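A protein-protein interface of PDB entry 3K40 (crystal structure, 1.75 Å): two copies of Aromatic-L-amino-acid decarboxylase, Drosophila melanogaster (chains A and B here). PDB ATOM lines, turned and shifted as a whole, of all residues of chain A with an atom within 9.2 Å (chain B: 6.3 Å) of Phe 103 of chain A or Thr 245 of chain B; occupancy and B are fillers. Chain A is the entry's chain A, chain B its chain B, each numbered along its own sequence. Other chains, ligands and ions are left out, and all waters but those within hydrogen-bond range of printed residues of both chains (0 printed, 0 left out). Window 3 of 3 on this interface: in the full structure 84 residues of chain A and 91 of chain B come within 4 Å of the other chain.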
ATOM      1  N   ALA A  99     -12.715  12.030 -32.422  1.00  0.00           N
ATOM      2  CA  ALA A  99     -13.904  12.796 -32.043  1.00  0.00           C
ATOM      3  C   ALA A  99     -13.794  13.436 -30.649  1.00  0.00           C
ATOM      4  O   ALA A  99     -12.931  13.074 -29.848  1.00  0.00           O
ATOM      5  CB  ALA A  99     -15.144  11.889 -32.106  1.00  0.00           C
ATOM      6  N   CYS A 100     -14.675  14.392 -30.365  1.00  0.00           N
ATOM      7  CA  CYS A 100     -14.881  14.822 -28.979  1.00  0.00           C
ATOM      8  C   CYS A 100     -16.369  14.880 -28.675  1.00  0.00           C
ATOM      9  O   CYS A 100     -17.198  14.942 -29.596  1.00  0.00           O
ATOM     10  CB  CYS A 100     -14.195  16.160 -28.700  1.00  0.00           C
ATOM     11  SG  CYS A 100     -15.067  17.586 -29.347  1.00  0.00           S
ATOM     12  N   ILE A 101     -16.705  14.853 -27.384  1.00  0.00           N
ATOM     13  CA  ILE A 101     -18.099  14.842 -26.942  1.00  0.00           C
ATOM     14  C   ILE A 101     -18.832  16.150 -27.291  1.00  0.00           C
ATOM     15  O   ILE A 101     -20.071  16.180 -27.394  1.00  0.00           O
ATOM     16  CB  ILE A 101     -18.195  14.479 -25.423  1.00  0.00           C
ATOM     17  CG1 ILE A 101     -19.448  13.644 -25.142  1.00  0.00           C
ATOM     18  CG2 ILE A 101     -18.127  15.717 -24.553  1.00  0.00           C
ATOM     19  CD1 ILE A 101     -19.368  12.807 -23.869  1.00  0.00           C
ATOM     20  N   GLY A 102     -18.057  17.224 -27.472  1.00  0.00           N
ATOM     21  CA  GLY A 102     -18.579  18.528 -27.872  1.00  0.00           C
ATOM     22  C   GLY A 102     -18.678  19.525 -26.728  1.00  0.00           C
ATOM     23  O   GLY A 102     -19.531  20.416 -26.747  1.00  0.00           O
ATOM     24  N   PHE A 103     -17.818  19.381 -25.721  1.00  0.00           N
ATOM     25  CA  PHE A 103     -17.836  20.335 -24.612  1.00  0.00           C
ATOM     26  C   PHE A 103     -17.334  21.692 -25.113  1.00  0.00           C
ATOM     27  O   PHE A 103     -18.053  22.696 -25.041  1.00  0.00           O
ATOM     28  CB  PHE A 103     -17.019  19.835 -23.418  1.00  0.00           C
ATOM     29  CG  PHE A 103     -16.863  20.854 -22.322  1.00  0.00           C
ATOM     30  CD1 PHE A 103     -15.607  21.396 -22.039  1.00  0.00           C
ATOM     31  CD2 PHE A 103     -17.967  21.277 -21.579  1.00  0.00           C
ATOM     32  CE1 PHE A 103     -15.448  22.342 -21.020  1.00  0.00           C
ATOM     33  CE2 PHE A 103     -17.823  22.222 -20.566  1.00  0.00           C
ATOM     34  CZ  PHE A 103     -16.562  22.756 -20.283  1.00  0.00           C
ATOM     35  N   THR A 104     -16.105  21.713 -25.626  1.00  0.00           N
ATOM     36  CA  THR A 104     -15.602  22.877 -26.355  1.00  0.00           C
ATOM     37  C   THR A 104     -16.208  22.850 -27.763  1.00  0.00           C
ATOM     38  O   THR A 104     -16.131  21.839 -28.470  1.00  0.00           O
ATOM     39  CB  THR A 104     -14.027  22.989 -26.316  1.00  0.00           C
ATOM     40  OG1 THR A 104     -13.500  23.305 -27.618  1.00  0.00           O
ATOM     41  CG2 THR A 104     -13.386  21.706 -25.771  1.00  0.00           C
ATOM     42  N   TRP A 105     -16.868  23.944 -28.128  1.00  0.00           N
ATOM     43  CA  TRP A 105     -17.621  24.041 -29.384  1.00  0.00           C
ATOM     44  C   TRP A 105     -16.836  23.550 -30.615  1.00  0.00           C
ATOM     45  O   TRP A 105     -15.750  24.063 -30.919  1.00  0.00           O
ATOM     46  CB  TRP A 105     -18.094  25.484 -29.576  1.00  0.00           C
ATOM     47  CG  TRP A 105     -18.504  25.800 -30.958  1.00  0.00           C
ATOM     48  CD1 TRP A 105     -17.771  26.471 -31.900  1.00  0.00           C
ATOM     49  CD2 TRP A 105     -19.746  25.461 -31.577  1.00  0.00           C
ATOM     50  NE1 TRP A 105     -18.485  26.571 -33.070  1.00  0.00           N
ATOM     51  CE2 TRP A 105     -19.702  25.959 -32.902  1.00  0.00           C
ATOM     52  CE3 TRP A 105     -20.895  24.787 -31.144  1.00  0.00           C
ATOM     53  CZ2 TRP A 105     -20.769  25.807 -33.797  1.00  0.00           C
ATOM     54  CZ3 TRP A 105     -21.949  24.632 -32.034  1.00  0.00           C
ATOM     55  CH2 TRP A 105     -21.879  25.140 -33.346  1.00  0.00           C
ATOM     56  N   ILE A 106     -17.393  22.557 -31.313  1.00  0.00           N
ATOM     57  CA  ILE A 106     -16.743  21.978 -32.497  1.00  0.00           C
ATOM     58  C   ILE A 106     -16.953  22.868 -33.731  1.00  0.00           C
ATOM     59  O   ILE A 106     -18.050  22.923 -34.302  1.00  0.00           O
ATOM     60  CB  ILE A 106     -17.225  20.519 -32.809  1.00  0.00           C
ATOM     61  CG1 ILE A 106     -17.329  19.683 -31.527  1.00  0.00           C
ATOM     62  CG2 ILE A 106     -16.295  19.845 -33.846  1.00  0.00           C
ATOM     63  CD1 ILE A 106     -17.875  18.285 -31.734  1.00  0.00           C
ATOM     64  N   PRO A 349     -24.335  21.699 -31.764  1.00  0.00           N
ATOM     65  CA  PRO A 349     -25.222  21.357 -32.878  1.00  0.00           C
ATOM     66  C   PRO A 349     -24.723  20.227 -33.793  1.00  0.00           C
ATOM     67  O   PRO A 349     -25.241  19.111 -33.691  1.00  0.00           O
ATOM     68  CB  PRO A 349     -25.373  22.695 -33.618  1.00  0.00           C
ATOM     69  CG  PRO A 349     -25.245  23.753 -32.499  1.00  0.00           C
ATOM     70  CD  PRO A 349     -24.640  23.051 -31.263  1.00  0.00           C
ATOM     71  N   ARG A 352     -20.996  16.563 -33.343  1.00  0.00           N
ATOM     72  CA  ARG A 352     -20.761  16.028 -32.005  1.00  0.00           C
ATOM     73  C   ARG A 352     -20.541  14.538 -32.110  1.00  0.00           C
ATOM     74  O   ARG A 352     -21.402  13.819 -32.625  1.00  0.00           O
ATOM     75  CB  ARG A 352     -21.940  16.326 -31.058  1.00  0.00           C
ATOM     76  CG  ARG A 352     -21.686  17.425 -30.020  1.00  0.00           C
ATOM     77  CD  ARG A 352     -21.377  18.804 -30.625  1.00  0.00           C
ATOM     78  NE  ARG A 352     -21.158  19.813 -29.580  1.00  0.00           N
ATOM     79  CZ  ARG A 352     -20.715  21.056 -29.793  1.00  0.00           C
ATOM     80  NH1 ARG A 352     -20.553  21.887 -28.765  1.00  0.00           N
ATOM     81  NH2 ARG A 352     -20.439  21.480 -31.027  1.00  0.00           N
ATOM     82  N   ARG A 353     -19.360  14.092 -31.676  1.00  0.00           N
ATOM     83  CA  ARG A 353     -19.003  12.672 -31.669  1.00  0.00           C
ATOM     84  C   ARG A 353     -18.696  12.071 -33.051  1.00  0.00           C
ATOM     85  O   ARG A 353     -18.483  10.874 -33.166  1.00  0.00           O
ATOM     86  CB  ARG A 353     -20.073  11.839 -30.950  1.00  0.00           C
ATOM     87  CG  ARG A 353     -20.370  12.280 -29.505  1.00  0.00           C
ATOM     88  CD  ARG A 353     -21.505  11.454 -28.959  1.00  0.00           C
ATOM     89  NE  ARG A 353     -21.512  11.343 -27.494  1.00  0.00           N
ATOM     90  CZ  ARG A 353     -22.020  12.253 -26.667  1.00  0.00           C
ATOM     91  NH1 ARG A 353     -22.543  13.377 -27.146  1.00  0.00           N
ATOM     92  NH2 ARG A 353     -21.996  12.049 -25.345  1.00  0.00           N
ATOM     93  N   TYR B  79     -11.062  23.719 -24.380  1.00  0.00           N
ATOM     94  CA  TYR B  79     -11.523  24.112 -23.029  1.00  0.00           C
ATOM     95  C   TYR B  79     -10.993  23.217 -21.935  1.00  0.00           C
ATOM     96  O   TYR B  79     -10.477  23.701 -20.934  1.00  0.00           O
ATOM     97  CB  TYR B  79     -13.065  24.292 -22.945  1.00  0.00           C
ATOM     98  CG  TYR B  79     -13.443  25.699 -23.355  1.00  0.00           C
ATOM     99  CD1 TYR B  79     -13.336  26.765 -22.455  1.00  0.00           C
ATOM    100  CD2 TYR B  79     -13.808  25.977 -24.671  1.00  0.00           C
ATOM    101  CE1 TYR B  79     -13.618  28.095 -22.859  1.00  0.00           C
ATOM    102  CE2 TYR B  79     -14.104  27.278 -25.080  1.00  0.00           C
ATOM    103  CZ  TYR B  79     -14.002  28.336 -24.172  1.00  0.00           C
ATOM    104  OH  TYR B  79     -14.283  29.639 -24.606  1.00  0.00           O
ATOM    105  N   PHE B  80     -11.101  21.907 -22.154  1.00  0.00           N
ATOM    106  CA  PHE B  80     -10.579  20.919 -21.235  1.00  0.00           C
ATOM    107  C   PHE B  80     -10.160  19.707 -22.060  1.00  0.00           C
ATOM    108  O   PHE B  80     -10.522  19.613 -23.254  1.00  0.00           O
ATOM    109  CB  PHE B  80     -11.636  20.518 -20.195  1.00  0.00           C
ATOM    110  CG  PHE B  80     -11.769  21.485 -19.036  1.00  0.00           C
ATOM    111  CD1 PHE B  80     -10.646  21.952 -18.344  1.00  0.00           C
ATOM    112  CD2 PHE B  80     -13.031  21.891 -18.613  1.00  0.00           C
ATOM    113  CE1 PHE B  80     -10.778  22.853 -17.259  1.00  0.00           C
ATOM    114  CE2 PHE B  80     -13.180  22.776 -17.535  1.00  0.00           C
ATOM    115  CZ  PHE B  80     -12.043  23.260 -16.851  1.00  0.00           C
ATOM    116  N   GLN B 190     -20.633  30.966 -11.234  1.00  0.00           N
ATOM    117  CA  GLN B 190     -19.616  30.348 -12.101  1.00  0.00           C
ATOM    118  C   GLN B 190     -19.929  28.873 -12.441  1.00  0.00           C
ATOM    119  O   GLN B 190     -19.078  28.199 -13.030  1.00  0.00           O
ATOM    120  CB  GLN B 190     -18.239  30.371 -11.422  1.00  0.00           C
ATOM    121  CG  GLN B 190     -17.653  31.745 -11.165  1.00  0.00           C
ATOM    122  CD  GLN B 190     -17.462  32.491 -12.425  1.00  0.00           C
ATOM    123  OE1 GLN B 190     -16.651  32.097 -13.275  1.00  0.00           O
ATOM    124  NE2 GLN B 190     -18.244  33.557 -12.609  1.00  0.00           N
ATOM    125  N   ALA B 191     -21.095  28.357 -12.035  1.00  0.00           N
ATOM    126  CA  ALA B 191     -21.448  26.953 -12.336  1.00  0.00           C
ATOM    127  C   ALA B 191     -21.641  26.785 -13.822  1.00  0.00           C
ATOM    128  O   ALA B 191     -21.876  27.762 -14.523  1.00  0.00           O
ATOM    129  CB  ALA B 191     -22.701  26.520 -11.616  1.00  0.00           C
ATOM    130  N   HIS B 192     -21.538  25.548 -14.305  1.00  0.00           N
ATOM    131  CA  HIS B 192     -21.627  25.324 -15.748  1.00  0.00           C
ATOM    132  C   HIS B 192     -23.078  25.480 -16.213  1.00  0.00           C
ATOM    133  O   HIS B 192     -23.991  25.212 -15.442  1.00  0.00           O
ATOM    134  CB  HIS B 192     -21.098  23.938 -16.079  1.00  0.00           C
ATOM    135  CG  HIS B 192     -21.093  23.626 -17.543  1.00  0.00           C
ATOM    136  ND1 HIS B 192     -21.983  22.745 -18.115  1.00  0.00           N
ATOM    137  CD2 HIS B 192     -20.321  24.088 -18.554  1.00  0.00           C
ATOM    138  CE1 HIS B 192     -21.761  22.672 -19.416  1.00  0.00           C
ATOM    139  NE2 HIS B 192     -20.757  23.477 -19.710  1.00  0.00           N
ATOM    140  N   SER B 193     -23.268  25.902 -17.470  1.00  0.00           N
ATOM    141  CA  SER B 193     -24.605  26.045 -18.062  1.00  0.00           C
ATOM    142  C   SER B 193     -25.474  24.804 -17.920  1.00  0.00           C
ATOM    143  O   SER B 193     -26.690  24.919 -17.997  1.00  0.00           O
ATOM    144  CB  SER B 193     -24.518  26.442 -19.540  1.00  0.00           C
ATOM    145  OG  SER B 193     -23.938  25.388 -20.301  1.00  0.00           O
ATOM    146  N   THR B 241     -19.624  23.409  -7.124  1.00  0.00           N
ATOM    147  CA  THR B 241     -18.721  23.130  -8.229  1.00  0.00           C
ATOM    148  C   THR B 241     -17.271  23.086  -7.759  1.00  0.00           C
ATOM    149  O   THR B 241     -16.770  24.076  -7.213  1.00  0.00           O
ATOM    150  CB  THR B 241     -18.899  24.159  -9.356  1.00  0.00           C
ATOM    151  OG1 THR B 241     -20.285  24.191  -9.769  1.00  0.00           O
ATOM    152  CG2 THR B 241     -18.012  23.793 -10.549  1.00  0.00           C
ATOM    153  N   GLY B 243     -13.999  22.961  -9.454  1.00  0.00           N
ATOM    154  CA  GLY B 243     -13.286  23.133 -10.717  1.00  0.00           C
ATOM    155  C   GLY B 243     -14.210  23.755 -11.743  1.00  0.00           C
ATOM    156  O   GLY B 243     -14.592  23.082 -12.709  1.00  0.00           O
ATOM    157  N   THR B 244     -14.558  25.038 -11.565  1.00  0.00           N
ATOM    158  CA  THR B 244     -15.438  25.744 -12.501  1.00  0.00           C
ATOM    159  C   THR B 244     -14.868  25.753 -13.937  1.00  0.00           C
ATOM    160  O   THR B 244     -13.660  25.734 -14.126  1.00  0.00           O
ATOM    161  CB  THR B 244     -15.656  27.198 -12.096  1.00  0.00           C
ATOM    162  OG1 THR B 244     -14.389  27.891 -12.088  1.00  0.00           O
ATOM    163  CG2 THR B 244     -16.344  27.261 -10.708  1.00  0.00           C
ATOM    164  N   THR B 245     -15.751  25.815 -14.935  1.00  0.00           N
ATOM    165  CA  THR B 245     -15.272  25.776 -16.315  1.00  0.00           C
ATOM    166  C   THR B 245     -14.428  26.992 -16.717  1.00  0.00           C
ATOM    167  O   THR B 245     -13.445  26.842 -17.443  1.00  0.00           O
ATOM    168  CB  THR B 245     -16.404  25.532 -17.319  1.00  0.00           C
ATOM    169  OG1 THR B 245     -17.338  26.627 -17.280  1.00  0.00           O
ATOM    170  CG2 THR B 245     -17.099  24.226 -17.005  1.00  0.00           C
ATOM    171  N   ASN B 246     -14.796  28.181 -16.227  1.00  0.00           N
ATOM    172  CA  ASN B 246     -14.097  29.416 -16.586  1.00  0.00           C
ATOM    173  C   ASN B 246     -12.643  29.462 -16.101  1.00  0.00           C
ATOM    174  O   ASN B 246     -11.716  29.795 -16.866  1.00  0.00           O
ATOM    175  CB  ASN B 246     -14.875  30.632 -16.049  1.00  0.00           C
ATOM    176  CG  ASN B 246     -16.049  31.003 -16.920  1.00  0.00           C
ATOM    177  OD1 ASN B 246     -16.103  30.631 -18.096  1.00  0.00           O
ATOM    178  ND2 ASN B 246     -16.996  31.766 -16.356  1.00  0.00           N
ATOM    179  N   SER B 247     -12.418  29.140 -14.837  1.00  0.00           N
ATOM    180  CA  SER B 247     -11.081  29.340 -14.242  1.00  0.00           C
ATOM    181  C   SER B 247     -10.601  28.208 -13.339  1.00  0.00           C
ATOM    182  O   SER B 247      -9.523  28.299 -12.725  1.00  0.00           O
ATOM    183  CB  SER B 247     -11.032  30.665 -13.482  1.00  0.00           C
ATOM    184  OG  SER B 247     -11.966  30.636 -12.417  1.00  0.00           O
ATOM    185  N   CYS B 248     -11.387  27.139 -13.264  1.00  0.00           N
ATOM    186  CA  CYS B 248     -11.121  26.010 -12.400  1.00  0.00           C
ATOM    187  C   CYS B 248     -11.000  26.461 -10.932  1.00  0.00           C
ATOM    188  O   CYS B 248     -10.086  26.054 -10.229  1.00  0.00           O
ATOM    189  CB  CYS B 248      -9.882  25.200 -12.854  1.00  0.00           C
ATOM    190  SG  CYS B 248      -9.761  23.536 -12.200  1.00  0.00           S
ATOM    191  N   ALA B 249     -11.953  27.289 -10.505  1.00  0.00           N
ATOM    192  CA  ALA B 249     -12.061  27.669  -9.090  1.00  0.00           C
ATOM    193  C   ALA B 249     -12.839  26.585  -8.357  1.00  0.00           C
ATOM    194  O   ALA B 249     -13.547  25.771  -8.997  1.00  0.00           O
ATOM    195  CB  ALA B 249     -12.759  28.997  -8.977  1.00  0.00           C
ATOM    196  N1  LLP B 302     -19.421  21.024 -15.210  1.00  0.00           N
ATOM    197  C2  LLP B 302     -18.056  21.183 -15.234  1.00  0.00           C
ATOM    198  C2' LLP B 302     -17.400  21.803 -14.025  1.00  0.00           C
ATOM    199  C3  LLP B 302     -17.295  20.765 -16.341  1.00  0.00           C
ATOM    200  O3  LLP B 302     -16.048  20.899 -16.314  1.00  0.00           O
ATOM    201  C4  LLP B 302     -17.958  20.182 -17.438  1.00  0.00           C
ATOM    202  C4' LLP B 302     -17.210  19.667 -18.654  1.00  0.00           C
ATOM    203  C5  LLP B 302     -19.356  20.052 -17.404  1.00  0.00           C
ATOM    204  C6  LLP B 302     -20.086  20.467 -16.301  1.00  0.00           C
ATOM    205  C5' LLP B 302     -20.119  19.435 -18.566  1.00  0.00           C
ATOM    206  OP4 LLP B 302     -19.867  18.030 -18.669  1.00  0.00           O
ATOM    207  P   LLP B 302     -20.466  17.095 -19.852  1.00  0.00           P
ATOM    208  OP1 LLP B 302     -19.781  17.645 -21.052  1.00  0.00           O
ATOM    209  OP2 LLP B 302     -19.980  15.794 -19.440  1.00  0.00           O
ATOM    210  OP3 LLP B 302     -21.927  17.384 -19.879  1.00  0.00           O
ATOM    211  N   LLP B 302     -12.868  13.404 -19.395  1.00  0.00           N
ATOM    212  CA  LLP B 302     -12.074  14.624 -19.599  1.00  0.00           C
ATOM    213  CB  LLP B 302     -12.583  15.810 -18.778  1.00  0.00           C
ATOM    214  CG  LLP B 302     -13.807  16.493 -19.431  1.00  0.00           C
ATOM    215  CD  LLP B 302     -14.316  17.664 -18.570  1.00  0.00           C
ATOM    216  CE  LLP B 302     -15.318  18.467 -19.326  1.00  0.00           C
ATOM    217  NZ  LLP B 302     -15.949  19.410 -18.391  1.00  0.00           N
ATOM    218  C   LLP B 302     -10.627  14.310 -19.282  1.00  0.00           C
ATOM    219  O   LLP B 302      -9.836  14.089 -20.174  1.00  0.00           O
ATOM    220  N   LEU B 405      -4.950  24.292 -15.772  1.00  0.00           N
ATOM    221  CA  LEU B 405      -5.474  25.473 -16.450  1.00  0.00           C
ATOM    222  C   LEU B 405      -4.777  26.751 -15.991  1.00  0.00           C
ATOM    223  O   LEU B 405      -4.673  27.001 -14.775  1.00  0.00           O
ATOM    224  CB  LEU B 405      -6.980  25.624 -16.153  1.00  0.00           C
ATOM    225  CG  LEU B 405      -7.624  26.924 -16.670  1.00  0.00           C
ATOM    226  CD1 LEU B 405      -7.624  26.961 -18.201  1.00  0.00           C
ATOM    227  CD2 LEU B 405      -9.065  26.991 -16.199  1.00  0.00           C
ATOM    228  N   ALA B 435     -12.313  33.241 -22.242  1.00  0.00           N
ATOM    229  CA  ALA B 435     -13.410  33.198 -21.278  1.00  0.00           C
ATOM    230  C   ALA B 435     -13.570  34.584 -20.661  1.00  0.00           C
ATOM    231  O   ALA B 435     -12.693  35.448 -20.819  1.00  0.00           O
ATOM    232  CB  ALA B 435     -13.159  32.162 -20.183  1.00  0.00           C
ATOM    233  N   ARG B 444      -7.307  31.384 -22.014  1.00  0.00           N
ATOM    234  CA  ARG B 444      -7.077  30.148 -21.258  1.00  0.00           C
ATOM    235  C   ARG B 444      -6.101  29.238 -21.986  1.00  0.00           C
ATOM    236  O   ARG B 444      -6.243  29.006 -23.199  1.00  0.00           O
ATOM    237  CB  ARG B 444      -8.369  29.340 -21.084  1.00  0.00           C
ATOM    238  CG  ARG B 444      -9.372  29.941 -20.089  1.00  0.00           C
ATOM    239  CD  ARG B 444     -10.708  29.240 -20.265  1.00  0.00           C
ATOM    240  NE  ARG B 444     -10.972  28.073 -19.425  1.00  0.00           N
ATOM    241  CZ  ARG B 444     -10.703  26.801 -19.723  1.00  0.00           C
ATOM    242  NH1 ARG B 444     -10.042  26.488 -20.838  1.00  0.00           N
ATOM    243  NH2 ARG B 444     -11.064  25.834 -18.873  1.00  0.00           N
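The backbone carbonyl oxygen (O) of Tyr 79 of chain B lies within hydrogen-bond range of the guanidinium group (NH1) of Arg 444 of chain B (2.8 Å).
The backbone carbonyl oxygen (O) of Thr 245 of chain B is in hydrogen-bond range of the guanidinium group (NH2) of Arg 444 of chain B, 3.0 Å away.
Phe 103 of chain A touches Tyr 79 of chain B.
Phe 80 of chain B touches Phe 103 of chain A.
NE2 of His 192 of chain B touches CE2 of Phe 103 of chain A, 3.3 Å away.
Phe 103 of chain A touches Thr 245 of chain B (CZ to CG2, 3.6 Å).
LLP 302 of chain B touches Phe 103 of chain A.
Thr 104 of chain A touches Tyr 79 of chain B (CG2 to N, 3.4 Å).
Of chain B, only Tyr 79 (3.6 Å), Phe 80 (3.4 Å), His 192 (3.3 Å), Thr 245 (3.6 Å) and LLP 302 (3.2 Å) come within 4 Å of Phe 103 of chain A.
Printed residues of chain B within 4 Å of Thr 104 of chain A: Tyr 79.
Printed residues of chain A within 4 Å of Tyr 79 of chain B: Phe 103 and Thr 104.
Printed residues of chain A within 4 Å of Phe 80 of chain B: Phe 103 (3.4 Å).
Printed residues of chain A within 4 Å of His 192 of chain B: Phe 103 (3.3 Å).
Gly 243 of chain B touches none of the printed residues of chain A.
Thr 245 of chain B touches just one residue of chain A: Phe 103 (3.6 Å).
Printed residues of chain A within 4 Å of LLP 302 of chain B: Phe 103 (3.2 Å).
Arg 444 of chain B touches none of the printed residues of chain A.
The nearest residue of chain B that does not touch Phe 103 of chain A is Arg 444 of chain B (6.0 Å).
The nearest residue of chain A that does not touch Thr 245 of chain B is Thr 104 of chain A (9.0 Å).
Of the 11 printed residues of chain A, 2 touch a printed residue of chain B.
No position is printed for both chains.
Of the 6 pairs that touch across the chains among the printed residues, none has its exchanged pair printed and touching as well.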
